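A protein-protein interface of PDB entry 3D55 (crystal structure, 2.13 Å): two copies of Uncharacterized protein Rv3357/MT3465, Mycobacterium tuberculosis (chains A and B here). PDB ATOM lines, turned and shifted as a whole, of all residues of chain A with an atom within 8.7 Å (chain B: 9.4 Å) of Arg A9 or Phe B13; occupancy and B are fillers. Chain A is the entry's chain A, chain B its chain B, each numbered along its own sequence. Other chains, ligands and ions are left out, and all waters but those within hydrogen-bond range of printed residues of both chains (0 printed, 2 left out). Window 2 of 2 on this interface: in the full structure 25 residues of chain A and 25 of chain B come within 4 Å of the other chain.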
ATOM      1  N   ILE A   3     -12.183  15.391  -4.493  1.00  0.00           N
ATOM      2  CA  ILE A   3     -13.376  15.633  -3.689  1.00  0.00           C
ATOM      3  C   ILE A   3     -13.495  17.127  -3.233  1.00  0.00           C
ATOM      4  O   ILE A   3     -12.584  17.968  -3.502  1.00  0.00           O
ATOM      5  CB  ILE A   3     -13.319  14.692  -2.462  1.00  0.00           C
ATOM      6  CG1 ILE A   3     -12.224  15.136  -1.490  1.00  0.00           C
ATOM      7  CG2 ILE A   3     -12.974  13.263  -2.902  1.00  0.00           C
ATOM      8  CD1 ILE A   3     -11.776  14.029  -0.539  1.00  0.00           C
ATOM      9  N   SER A   4     -14.597  17.467  -2.546  1.00  0.00           N
ATOM     10  CA  SER A   4     -14.764  18.829  -1.981  1.00  0.00           C
ATOM     11  C   SER A   4     -14.255  18.861  -0.567  1.00  0.00           C
ATOM     12  O   SER A   4     -14.260  17.830   0.099  1.00  0.00           O
ATOM     13  CB  SER A   4     -16.233  19.249  -1.968  1.00  0.00           C
ATOM     14  OG  SER A   4     -16.915  18.620  -0.903  1.00  0.00           O
ATOM     15  N   ALA A   5     -13.893  20.047  -0.077  1.00  0.00           N
ATOM     16  CA  ALA A   5     -13.571  20.253   1.363  1.00  0.00           C
ATOM     17  C   ALA A   5     -14.593  19.753   2.358  1.00  0.00           C
ATOM     18  O   ALA A   5     -14.218  19.080   3.318  1.00  0.00           O
ATOM     19  CB  ALA A   5     -13.255  21.691   1.644  1.00  0.00           C
ATOM     20  N   SER A   6     -15.888  20.075   2.178  1.00  0.00           N
ATOM     21  CA  SER A   6     -16.868  19.438   3.091  1.00  0.00           C
ATOM     22  C   SER A   6     -16.854  17.931   2.872  1.00  0.00           C
ATOM     23  O   SER A   6     -16.772  17.189   3.805  1.00  0.00           O
ATOM     24  CB  SER A   6     -18.295  19.985   2.911  1.00  0.00           C
ATOM     25  OG  SER A   6     -18.608  20.026   1.534  1.00  0.00           O
ATOM     26  N   GLU A   7     -16.894  17.467   1.614  1.00  0.00           N
ATOM     27  CA  GLU A   7     -16.840  16.015   1.404  1.00  0.00           C
ATOM     28  C   GLU A   7     -15.540  15.504   2.105  1.00  0.00           C
ATOM     29  O   GLU A   7     -15.547  14.512   2.803  1.00  0.00           O
ATOM     30  CB  GLU A   7     -16.854  15.710  -0.082  1.00  0.00           C
ATOM     31  CG  GLU A   7     -16.967  14.232  -0.469  1.00  0.00           C
ATOM     32  CD  GLU A   7     -16.852  14.053  -1.993  1.00  0.00           C
ATOM     33  OE1 GLU A   7     -16.730  12.905  -2.464  1.00  0.00           O
ATOM     34  OE2 GLU A   7     -16.873  15.076  -2.716  1.00  0.00           O
ATOM     35  N   ALA A   8     -14.460  16.268   1.997  1.00  0.00           N
ATOM     36  CA  ALA A   8     -13.153  15.836   2.569  1.00  0.00           C
ATOM     37  C   ALA A   8     -13.102  15.960   4.108  1.00  0.00           C
ATOM     38  O   ALA A   8     -12.444  15.200   4.794  1.00  0.00           O
ATOM     39  CB  ALA A   8     -11.983  16.616   1.868  1.00  0.00           C
ATOM     40  N   ARG A   9     -13.812  16.957   4.638  1.00  0.00           N
ATOM     41  CA  ARG A   9     -13.952  17.054   6.068  1.00  0.00           C
ATOM     42  C   ARG A   9     -14.694  15.864   6.708  1.00  0.00           C
ATOM     43  O   ARG A   9     -14.212  15.242   7.640  1.00  0.00           O
ATOM     44  CB  ARG A   9     -14.606  18.377   6.465  1.00  0.00           C
ATOM     45  CG  ARG A   9     -15.036  18.301   7.913  1.00  0.00           C
ATOM     46  CD  ARG A   9     -15.319  19.654   8.476  1.00  0.00           C
ATOM     47  NE  ARG A   9     -16.452  20.278   7.797  1.00  0.00           N
ATOM     48  CZ  ARG A   9     -16.827  21.534   8.002  1.00  0.00           C
ATOM     49  NH1 ARG A   9     -16.147  22.288   8.860  1.00  0.00           N
ATOM     50  NH2 ARG A   9     -17.860  22.041   7.328  1.00  0.00           N
ATOM     51  N   GLN A  10     -15.854  15.493   6.198  1.00  0.00           N
ATOM     52  CA  GLN A  10     -16.547  14.461   6.954  1.00  0.00           C
ATOM     53  C   GLN A  10     -15.873  13.105   6.713  1.00  0.00           C
ATOM     54  O   GLN A  10     -15.706  12.296   7.643  1.00  0.00           O
ATOM     55  CB  GLN A  10     -18.021  14.466   6.637  1.00  0.00           C
ATOM     56  CG  GLN A  10     -18.831  14.241   7.864  1.00  0.00           C
ATOM     57  CD  GLN A  10     -20.258  13.996   7.517  1.00  0.00           C
ATOM     58  OE1 GLN A  10     -20.620  12.870   7.159  1.00  0.00           O
ATOM     59  NE2 GLN A  10     -21.096  15.056   7.595  1.00  0.00           N
ATOM     60  N   ARG A  11     -15.346  12.943   5.488  1.00  0.00           N
ATOM     61  CA  ARG A  11     -14.673  11.705   5.128  1.00  0.00           C
ATOM     62  C   ARG A  11     -13.186  11.631   5.543  1.00  0.00           C
ATOM     63  O   ARG A  11     -12.500  10.700   5.148  1.00  0.00           O
ATOM     64  CB  ARG A  11     -14.902  11.408   3.635  1.00  0.00           C
ATOM     65  CG  ARG A  11     -16.257  10.702   3.349  1.00  0.00           C
ATOM     66  CD  ARG A  11     -16.794  10.102   4.706  1.00  0.00           C
ATOM     67  NE  ARG A  11     -17.916   9.169   4.612  1.00  0.00           N
ATOM     68  CZ  ARG A  11     -19.185   9.466   4.923  1.00  0.00           C
ATOM     69  NH1 ARG A  11     -19.516  10.679   5.347  1.00  0.00           N
ATOM     70  NH2 ARG A  11     -20.126   8.525   4.813  1.00  0.00           N
ATOM     71  N   LEU A  12     -12.682  12.590   6.328  1.00  0.00           N
ATOM     72  CA  LEU A  12     -11.223  12.661   6.583  1.00  0.00           C
ATOM     73  C   LEU A  12     -10.512  11.417   7.102  1.00  0.00           C
ATOM     74  O   LEU A  12      -9.386  11.187   6.702  1.00  0.00           O
ATOM     75  CB  LEU A  12     -10.766  13.931   7.371  1.00  0.00           C
ATOM     76  CG  LEU A  12      -9.262  14.083   7.779  1.00  0.00           C
ATOM     77  CD1 LEU A  12      -8.334  14.124   6.572  1.00  0.00           C
ATOM     78  CD2 LEU A  12      -8.962  15.355   8.600  1.00  0.00           C
ATOM     79  N   PHE A  13     -11.077  10.662   8.039  1.00  0.00           N
ATOM     80  CA  PHE A  13     -10.358   9.448   8.586  1.00  0.00           C
ATOM     81  C   PHE A  13     -10.160   8.284   7.555  1.00  0.00           C
ATOM     82  O   PHE A  13      -9.118   7.660   7.519  1.00  0.00           O
ATOM     83  CB  PHE A  13     -11.068   8.874   9.826  1.00  0.00           C
ATOM     84  CG  PHE A  13     -10.717   9.586  11.104  1.00  0.00           C
ATOM     85  CD1 PHE A  13      -9.821   8.999  12.030  1.00  0.00           C
ATOM     86  CD2 PHE A  13     -11.176  10.898  11.329  1.00  0.00           C
ATOM     87  CE1 PHE A  13      -9.450   9.705  13.181  1.00  0.00           C
ATOM     88  CE2 PHE A  13     -10.826  11.633  12.495  1.00  0.00           C
ATOM     89  CZ  PHE A  13      -9.981  11.044  13.422  1.00  0.00           C
ATOM     90  N   PRO A  14     -11.207   7.976   6.766  1.00  0.00           N
ATOM     91  CA  PRO A  14     -11.023   6.915   5.763  1.00  0.00           C
ATOM     92  C   PRO A  14     -10.030   7.389   4.679  1.00  0.00           C
ATOM     93  O   PRO A  14      -9.290   6.605   4.179  1.00  0.00           O
ATOM     94  CB  PRO A  14     -12.387   6.726   5.148  1.00  0.00           C
ATOM     95  CG  PRO A  14     -13.274   7.834   5.737  1.00  0.00           C
ATOM     96  CD  PRO A  14     -12.622   8.336   6.983  1.00  0.00           C
ATOM     97  N   LEU A  15     -10.035   8.672   4.402  1.00  0.00           N
ATOM     98  CA  LEU A  15      -9.051   9.325   3.488  1.00  0.00           C
ATOM     99  C   LEU A  15      -7.654   9.062   3.942  1.00  0.00           C
ATOM    100  O   LEU A  15      -6.817   8.685   3.135  1.00  0.00           O
ATOM    101  CB  LEU A  15      -9.392  10.795   3.275  1.00  0.00           C
ATOM    102  CG  LEU A  15     -10.643  10.980   2.374  1.00  0.00           C
ATOM    103  CD1 LEU A  15     -11.135  12.429   2.237  1.00  0.00           C
ATOM    104  CD2 LEU A  15     -10.606  10.305   1.023  1.00  0.00           C
ATOM    105  N   ILE A  28      -8.355  17.902  -2.832  1.00  0.00           N
ATOM    106  CA  ILE A  28      -9.478  18.490  -2.131  1.00  0.00           C
ATOM    107  C   ILE A  28      -9.702  19.883  -2.712  1.00  0.00           C
ATOM    108  O   ILE A  28      -8.780  20.749  -2.696  1.00  0.00           O
ATOM    109  CB  ILE A  28      -9.189  18.644  -0.632  1.00  0.00           C
ATOM    110  CG1 ILE A  28      -9.010  17.275  -0.004  1.00  0.00           C
ATOM    111  CG2 ILE A  28     -10.347  19.435   0.040  1.00  0.00           C
ATOM    112  CD1 ILE A  28      -8.334  17.268   1.320  1.00  0.00           C
ATOM    113  N   THR A  29     -10.912  20.068  -3.236  1.00  0.00           N
ATOM    114  CA  THR A  29     -11.418  21.347  -3.745  1.00  0.00           C
ATOM    115  C   THR A  29     -11.983  22.235  -2.634  1.00  0.00           C
ATOM    116  O   THR A  29     -12.492  21.757  -1.647  1.00  0.00           O
ATOM    117  CB  THR A  29     -12.484  21.069  -4.858  1.00  0.00           C
ATOM    118  OG1 THR A  29     -11.811  20.996  -6.122  1.00  0.00           O
ATOM    119  CG2 THR A  29     -13.594  22.126  -4.914  1.00  0.00           C
ATOM    120  N   SER A  30     -11.827  23.540  -2.756  1.00  0.00           N
ATOM    121  CA  SER A  30     -12.480  24.483  -1.836  1.00  0.00           C
ATOM    122  C   SER A  30     -12.239  25.806  -2.468  1.00  0.00           C
ATOM    123  O   SER A  30     -11.257  25.962  -3.169  1.00  0.00           O
ATOM    124  CB  SER A  30     -11.890  24.467  -0.416  1.00  0.00           C
ATOM    125  OG  SER A  30     -10.985  25.552  -0.187  1.00  0.00           O
ATOM    126  N   ARG A  31     -13.133  26.763  -2.219  1.00  0.00           N
ATOM    127  CA  ARG A  31     -13.015  28.107  -2.806  1.00  0.00           C
ATOM    128  C   ARG A  31     -11.857  28.885  -2.153  1.00  0.00           C
ATOM    129  O   ARG A  31     -11.525  29.982  -2.558  1.00  0.00           O
ATOM    130  CB  ARG A  31     -14.379  28.890  -2.791  1.00  0.00           C
ATOM    131  CG  ARG A  31     -15.595  28.216  -2.064  1.00  0.00           C
ATOM    132  CD  ARG A  31     -16.336  27.105  -2.916  1.00  0.00           C
ATOM    133  NE  ARG A  31     -17.154  26.156  -2.126  1.00  0.00           N
ATOM    134  CZ  ARG A  31     -16.788  25.532  -0.988  1.00  0.00           C
ATOM    135  NH1 ARG A  31     -15.577  25.689  -0.437  1.00  0.00           N
ATOM    136  NH2 ARG A  31     -17.647  24.727  -0.384  1.00  0.00           N
ATOM    137  N   ALA A  32     -11.213  28.263  -1.177  1.00  0.00           N
ATOM    138  CA  ALA A  32     -10.137  28.861  -0.395  1.00  0.00           C
ATOM    139  C   ALA A  32      -8.744  28.353  -0.857  1.00  0.00           C
ATOM    140  O   ALA A  32      -7.702  28.617  -0.206  1.00  0.00           O
ATOM    141  CB  ALA A  32     -10.373  28.527   1.079  1.00  0.00           C
ATOM    142  N   GLY A  33      -8.724  27.629  -1.978  1.00  0.00           N
ATOM    143  CA  GLY A  33      -7.511  26.956  -2.455  1.00  0.00           C
ATOM    144  C   GLY A  33      -7.713  25.433  -2.488  1.00  0.00           C
ATOM    145  O   GLY A  33      -8.495  24.884  -1.748  1.00  0.00           O
ATOM    146  N   ALA A  35      -6.096  21.617  -2.111  1.00  0.00           N
ATOM    147  CA  ALA A  35      -5.080  21.028  -1.286  1.00  0.00           C
ATOM    148  C   ALA A  35      -4.983  19.570  -1.705  1.00  0.00           C
ATOM    149  O   ALA A  35      -5.885  19.081  -2.321  1.00  0.00           O
ATOM    150  CB  ALA A  35      -5.426  21.195   0.168  1.00  0.00           C
ATOM    151  N   ALA B   5      -5.605  13.949  13.668  1.00  0.00           N
ATOM    152  CA  ALA B   5      -6.645  13.909  12.670  1.00  0.00           C
ATOM    153  C   ALA B   5      -7.947  14.568  13.177  1.00  0.00           C
ATOM    154  O   ALA B   5      -8.547  15.398  12.466  1.00  0.00           O
ATOM    155  CB  ALA B   5      -6.851  12.440  12.192  1.00  0.00           C
ATOM    156  N   SER B   6      -8.346  14.282  14.425  1.00  0.00           N
ATOM    157  CA  SER B   6      -9.611  14.857  14.954  1.00  0.00           C
ATOM    158  C   SER B   6      -9.494  16.365  14.943  1.00  0.00           C
ATOM    159  O   SER B   6     -10.377  17.035  14.457  1.00  0.00           O
ATOM    160  CB  SER B   6      -9.997  14.424  16.398  1.00  0.00           C
ATOM    161  OG  SER B   6      -9.096  13.527  17.015  1.00  0.00           O
ATOM    162  N   GLU B   7      -8.385  16.902  15.433  1.00  0.00           N
ATOM    163  CA  GLU B   7      -8.241  18.361  15.366  1.00  0.00           C
ATOM    164  C   GLU B   7      -8.292  18.834  13.902  1.00  0.00           C
ATOM    165  O   GLU B   7      -8.910  19.873  13.590  1.00  0.00           O
ATOM    166  CB  GLU B   7      -6.974  18.817  16.028  1.00  0.00           C
ATOM    167  CG  GLU B   7      -6.185  19.764  15.181  1.00  0.00           C
ATOM    168  CD  GLU B   7      -5.396  20.760  15.993  1.00  0.00           C
ATOM    169  OE1 GLU B   7      -4.815  20.313  16.986  1.00  0.00           O
ATOM    170  OE2 GLU B   7      -5.372  21.986  15.669  1.00  0.00           O
ATOM    171  N   ALA B   8      -7.734  18.012  12.996  1.00  0.00           N
ATOM    172  CA  ALA B   8      -7.664  18.350  11.547  1.00  0.00           C
ATOM    173  C   ALA B   8      -9.037  18.380  10.913  1.00  0.00           C
ATOM    174  O   ALA B   8      -9.343  19.248  10.075  1.00  0.00           O
ATOM    175  CB  ALA B   8      -6.749  17.308  10.793  1.00  0.00           C
ATOM    176  N   ARG B   9      -9.887  17.427  11.293  1.00  0.00           N
ATOM    177  CA  ARG B   9     -11.172  17.267  10.595  1.00  0.00           C
ATOM    178  C   ARG B   9     -12.036  18.448  10.994  1.00  0.00           C
ATOM    179  O   ARG B   9     -12.751  19.052  10.162  1.00  0.00           O
ATOM    180  CB  ARG B   9     -11.786  15.896  10.898  1.00  0.00           C
ATOM    181  CG  ARG B   9     -13.061  15.545  10.159  1.00  0.00           C
ATOM    182  CD  ARG B   9     -14.155  15.371  11.197  1.00  0.00           C
ATOM    183  NE  ARG B   9     -13.901  14.197  12.019  1.00  0.00           N
ATOM    184  CZ  ARG B   9     -14.442  12.995  11.811  1.00  0.00           C
ATOM    185  NH1 ARG B   9     -15.334  12.793  10.812  1.00  0.00           N
ATOM    186  NH2 ARG B   9     -14.117  11.983  12.610  1.00  0.00           N
ATOM    187  N   GLN B  10     -11.843  18.839  12.250  1.00  0.00           N
ATOM    188  CA  GLN B  10     -12.476  20.002  12.837  1.00  0.00           C
ATOM    189  C   GLN B  10     -12.138  21.251  12.068  1.00  0.00           C
ATOM    190  O   GLN B  10     -13.018  21.917  11.485  1.00  0.00           O
ATOM    191  CB  GLN B  10     -11.923  20.125  14.268  1.00  0.00           C
ATOM    192  CG  GLN B  10     -12.667  21.008  15.227  1.00  0.00           C
ATOM    193  CD  GLN B  10     -14.146  21.086  14.925  1.00  0.00           C
ATOM    194  OE1 GLN B  10     -14.854  20.065  14.823  1.00  0.00           O
ATOM    195  NE2 GLN B  10     -14.632  22.308  14.786  1.00  0.00           N
ATOM    196  N   ARG B  11     -10.839  21.535  12.065  1.00  0.00           N
ATOM    197  CA  ARG B  11     -10.248  22.726  11.492  1.00  0.00           C
ATOM    198  C   ARG B  11      -9.862  22.614   9.967  1.00  0.00           C
ATOM    199  O   ARG B  11      -8.982  23.321   9.491  1.00  0.00           O
ATOM    200  CB  ARG B  11      -9.047  23.145  12.378  1.00  0.00           C
ATOM    201  CG  ARG B  11      -9.419  23.561  13.849  1.00  0.00           C
ATOM    202  CD  ARG B  11      -8.992  22.592  14.966  1.00  0.00           C
ATOM    203  NE  ARG B  11      -9.777  22.845  16.205  1.00  0.00           N
ATOM    204  CZ  ARG B  11      -9.644  22.245  17.402  1.00  0.00           C
ATOM    205  NH1 ARG B  11      -8.740  21.301  17.638  1.00  0.00           N
ATOM    206  NH2 ARG B  11     -10.445  22.610  18.387  1.00  0.00           N
ATOM    207  N   LEU B  12     -10.503  21.703   9.222  1.00  0.00           N
ATOM    208  CA  LEU B  12     -10.040  21.417   7.838  1.00  0.00           C
ATOM    209  C   LEU B  12      -9.967  22.681   6.998  1.00  0.00           C
ATOM    210  O   LEU B  12      -8.912  23.023   6.439  1.00  0.00           O
ATOM    211  CB  LEU B  12     -10.883  20.330   7.136  1.00  0.00           C
ATOM    212  CG  LEU B  12     -10.174  19.950   5.834  1.00  0.00           C
ATOM    213  CD1 LEU B  12      -8.758  19.351   6.152  1.00  0.00           C
ATOM    214  CD2 LEU B  12     -10.978  19.063   4.930  1.00  0.00           C
ATOM    215  N   PHE B  13     -11.103  23.379   6.935  1.00  0.00           N
ATOM    216  CA  PHE B  13     -11.238  24.646   6.213  1.00  0.00           C
ATOM    217  C   PHE B  13     -10.177  25.694   6.466  1.00  0.00           C
ATOM    218  O   PHE B  13      -9.545  26.181   5.516  1.00  0.00           O
ATOM    219  CB  PHE B  13     -12.644  25.234   6.455  1.00  0.00           C
ATOM    220  CG  PHE B  13     -13.697  24.555   5.687  1.00  0.00           C
ATOM    221  CD1 PHE B  13     -14.281  23.385   6.168  1.00  0.00           C
ATOM    222  CD2 PHE B  13     -14.116  25.061   4.462  1.00  0.00           C
ATOM    223  CE1 PHE B  13     -15.256  22.721   5.428  1.00  0.00           C
ATOM    224  CE2 PHE B  13     -15.089  24.420   3.731  1.00  0.00           C
ATOM    225  CZ  PHE B  13     -15.668  23.251   4.220  1.00  0.00           C
ATOM    226  N   PRO B  14      -9.984  26.084   7.734  1.00  0.00           N
ATOM    227  CA  PRO B  14      -8.840  26.933   8.114  1.00  0.00           C
ATOM    228  C   PRO B  14      -7.458  26.257   7.848  1.00  0.00           C
ATOM    229  O   PRO B  14      -6.479  26.926   7.558  1.00  0.00           O
ATOM    230  CB  PRO B  14      -9.029  27.103   9.624  1.00  0.00           C
ATOM    231  CG  PRO B  14     -10.444  26.850   9.867  1.00  0.00           C
ATOM    232  CD  PRO B  14     -10.869  25.811   8.893  1.00  0.00           C
ATOM    233  N   LEU B  15      -7.373  24.941   7.981  1.00  0.00           N
ATOM    234  CA  LEU B  15      -6.116  24.255   7.595  1.00  0.00           C
ATOM    235  C   LEU B  15      -5.875  24.403   6.072  1.00  0.00           C
ATOM    236  O   LEU B  15      -4.753  24.696   5.663  1.00  0.00           O
ATOM    237  CB  LEU B  15      -6.147  22.766   7.975  1.00  0.00           C
ATOM    238  CG  LEU B  15      -5.927  22.455   9.447  1.00  0.00           C
ATOM    239  CD1 LEU B  15      -5.945  20.928   9.634  1.00  0.00           C
ATOM    240  CD2 LEU B  15      -4.665  23.121   9.992  1.00  0.00           C
ATOM    241  N   ILE B  16      -6.936  24.244   5.259  1.00  0.00           N
ATOM    242  CA  ILE B  16      -6.862  24.386   3.790  1.00  0.00           C
ATOM    243  C   ILE B  16      -6.423  25.785   3.301  1.00  0.00           C
ATOM    244  O   ILE B  16      -5.621  25.891   2.376  1.00  0.00           O
ATOM    245  CB  ILE B  16      -8.158  24.008   3.087  1.00  0.00           C
ATOM    246  CG1 ILE B  16      -8.277  22.503   2.921  1.00  0.00           C
ATOM    247  CG2 ILE B  16      -8.199  24.551   1.587  1.00  0.00           C
ATOM    248  CD1 ILE B  16      -9.638  22.000   2.811  1.00  0.00           C
ATOM    249  N   GLU B  17      -7.031  26.845   3.847  1.00  0.00           N
ATOM    250  CA  GLU B  17      -6.725  28.249   3.540  1.00  0.00           C
ATOM    251  C   GLU B  17      -5.236  28.474   3.868  1.00  0.00           C
ATOM    252  O   GLU B  17      -4.491  29.196   3.204  1.00  0.00           O
ATOM    253  CB  GLU B  17      -7.618  29.079   4.517  1.00  0.00           C
ATOM    254  CG  GLU B  17      -8.126  30.476   4.140  1.00  0.00           C
ATOM    255  CD  GLU B  17      -9.126  31.041   5.246  1.00  0.00           C
ATOM    256  OE1 GLU B  17     -10.052  31.837   4.919  1.00  0.00           O
ATOM    257  OE2 GLU B  17      -8.976  30.670   6.454  1.00  0.00           O
ATOM    258  N   GLN B  18      -4.809  27.846   4.937  1.00  0.00           N
ATOM    259  CA  GLN B  18      -3.535  28.115   5.575  1.00  0.00           C
ATOM    260  C   GLN B  18      -2.390  27.435   4.842  1.00  0.00           C
ATOM    261  O   GLN B  18      -1.285  28.001   4.673  1.00  0.00           O
ATOM    262  CB  GLN B  18      -3.554  27.593   7.006  1.00  0.00           C
ATOM    263  CG  GLN B  18      -2.142  27.616   7.675  1.00  0.00           C
ATOM    264  CD  GLN B  18      -2.154  26.973   9.043  1.00  0.00           C
ATOM    265  OE1 GLN B  18      -1.213  26.247   9.456  1.00  0.00           O
ATOM    266  NE2 GLN B  18      -3.249  27.152   9.724  1.00  0.00           N
ATOM    267  N   VAL B  19      -2.643  26.193   4.449  1.00  0.00           N
ATOM    268  CA  VAL B  19      -1.711  25.496   3.570  1.00  0.00           C
ATOM    269  C   VAL B  19      -1.512  26.287   2.233  1.00  0.00           C
ATOM    270  O   VAL B  19      -0.437  26.266   1.648  1.00  0.00           O
ATOM    271  CB  VAL B  19      -2.211  24.057   3.443  1.00  0.00           C
ATOM    272  CG1 VAL B  19      -2.600  23.723   2.114  1.00  0.00           C
ATOM    273  CG2 VAL B  19      -1.325  23.069   4.237  1.00  0.00           C
ATOM    274  N   ASN B  20      -2.530  27.033   1.800  1.00  0.00           N
ATOM    275  CA  ASN B  20      -2.440  27.808   0.568  1.00  0.00           C
ATOM    276  C   ASN B  20      -1.888  29.232   0.822  1.00  0.00           C
ATOM    277  O   ASN B  20      -1.064  29.704   0.065  1.00  0.00           O
ATOM    278  CB  ASN B  20      -3.795  27.913  -0.127  1.00  0.00           C
ATOM    279  CG  ASN B  20      -4.076  26.759  -1.084  1.00  0.00           C
ATOM    280  OD1 ASN B  20      -3.758  26.842  -2.285  1.00  0.00           O
ATOM    281  ND2 ASN B  20      -4.659  25.688  -0.572  1.00  0.00           N
ATOM    282  N   THR B  21      -2.393  29.933   1.840  1.00  0.00           N
ATOM    283  CA  THR B  21      -1.747  31.205   2.325  1.00  0.00           C
ATOM    284  C   THR B  21      -0.313  31.079   2.781  1.00  0.00           C
ATOM    285  O   THR B  21       0.523  31.845   2.359  1.00  0.00           O
ATOM    286  CB  THR B  21      -2.502  31.766   3.508  1.00  0.00           C
ATOM    287  OG1 THR B  21      -3.895  31.603   3.239  1.00  0.00           O
ATOM    288  CG2 THR B  21      -2.138  33.295   3.860  1.00  0.00           C
ATOM    289  N   LEU B  37      -0.971  17.310   4.616  1.00  0.00           N
ATOM    290  CA  LEU B  37      -1.877  18.061   3.865  1.00  0.00           C
ATOM    291  C   LEU B  37      -1.034  19.245   3.423  1.00  0.00           C
ATOM    292  O   LEU B  37      -0.408  19.855   4.277  1.00  0.00           O
ATOM    293  CB  LEU B  37      -3.060  18.546   4.748  1.00  0.00           C
ATOM    294  CG  LEU B  37      -3.990  19.435   4.023  1.00  0.00           C
ATOM    295  CD1 LEU B  37      -4.936  18.611   2.975  1.00  0.00           C
ATOM    296  CD2 LEU B  37      -4.794  20.379   5.073  1.00  0.00           C
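The backbone carbonyl oxygen (O) of Gln A10 sits at hydrogen-bond distance from the guanidinium group (NH1) of Arg B9 (3.2 Å).
The side-chain hydroxyl (OG) of Ser A6 lies within hydrogen-bond range of the side-chain hydroxyl (OG) of Ser A4 (3.3 Å).
The guanidinium group (NH1) of Arg A11 lies within hydrogen-bond range of the side-chain amide oxygen (OE1) of Gln A10, at 3.1 Å.
The backbone carbonyl oxygen (O) of Gly A33 sits at hydrogen-bond distance from the side-chain hydroxyl (OG) of Ser A30, at 3.0 Å.
The backbone carbonyl oxygen (O) of Ala A35 sits at hydrogen-bond distance from the backbone NH (N) of Ile A28 (2.8 Å).
The backbone NH of Ala A32 lies within hydrogen-bond range of the side-chain hydroxyl of Ser A30 (2.9 Å).
The side-chain amide nitrogen of Asn B20 sits at hydrogen-bond distance from the backbone carbonyl oxygen of Ile B16 (3.1 Å).
Among the printed residues, pairs that only touch across the chains: Ala A5 with Leu B12, Ala A5 with Phe B13, Ala A5 with Ile B16, Ser A6 with Phe B13, Ala A8 with Leu B12, Arg A9 with Arg B9, Arg A9 with Leu B12, Arg A9 with Phe B13, Leu A12 with Ala B5, Leu A12 with Ala B8, Leu A12 with Arg B9, Phe A13 with Ala B5, Phe A13 with Ser B6, Phe A13 with Arg B9, Ile A28 with Ile B16, Ser A30 with Ile B16, Ala A32 with Glu B17, Ala A32 with Asn B20, Gly A33 with Ile B16, Gly A33 with Asn B20 and Ala A35 with Leu B37.
Of chain B, only Arg B9, Leu B12 and Phe B13 come within 4 Å of Arg A9.
Of chain A, only Ala A5 (3.9 Å), Ser A6 (3.8 Å) and Arg A9 (3.2 Å) come within 4 Å of Phe B13.
Of chain B, only Phe B13 comes within 4 Å of Ser A6.
Of chain B, only Leu B12 (3.8 Å) comes within 4 Å of Ala A8.
Printed residues of chain A within 4 Å of Arg B9: Arg A9 (2.8 Å), Gln A10 (3.2 Å), Leu A12 (3.5 Å) and Phe A13 (3.3 Å).
Of the printed residues of chain A, Ala B5 touches Leu A12 and Phe A13.
Of the printed residues of chain A, Leu B37 touches Ala A35 (3.8 Å).
The nearest printed residue of chain B that does not touch Ala A5 is Arg B9 (7.0 Å).
Printed residues of chain B that touch a printed residue of chain A: Ala B5, Ser B6, Ala B8, Arg B9, Leu B12, Phe B13, Ile B16, Glu B17, Asn B20 and Leu B37.
Hydrophobic or aromatic side chains of chain A that line the printed part of chain B: Ala A5, Leu A12, Phe A13, Ile A28 and Ala A35.
Among the printed residues, 22 pairs touch across the chains.
Among the printed residues, no Asp or Glu carboxylate lies within 4 Å of a Lys or Arg side-chain nitrogen of the other chain.
Ser A6 touches Phe B13, and with the chains exchanged Phe A13 touches Ser B6.
Arg A9 touches Leu B12, and with the chains exchanged Leu A12 touches Arg B9.
Arg A9 touches Phe B13, and with the chains exchanged Phe A13 touches Arg B9.
Gln A10 touches Arg B9, but with the chains exchanged Arg A9 does not touch Gln B10 (4.1 Å).
Positions printed for both chains: 5, 6, 7, 8, 9, 10, 11, 12, 13, 14 and 15.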
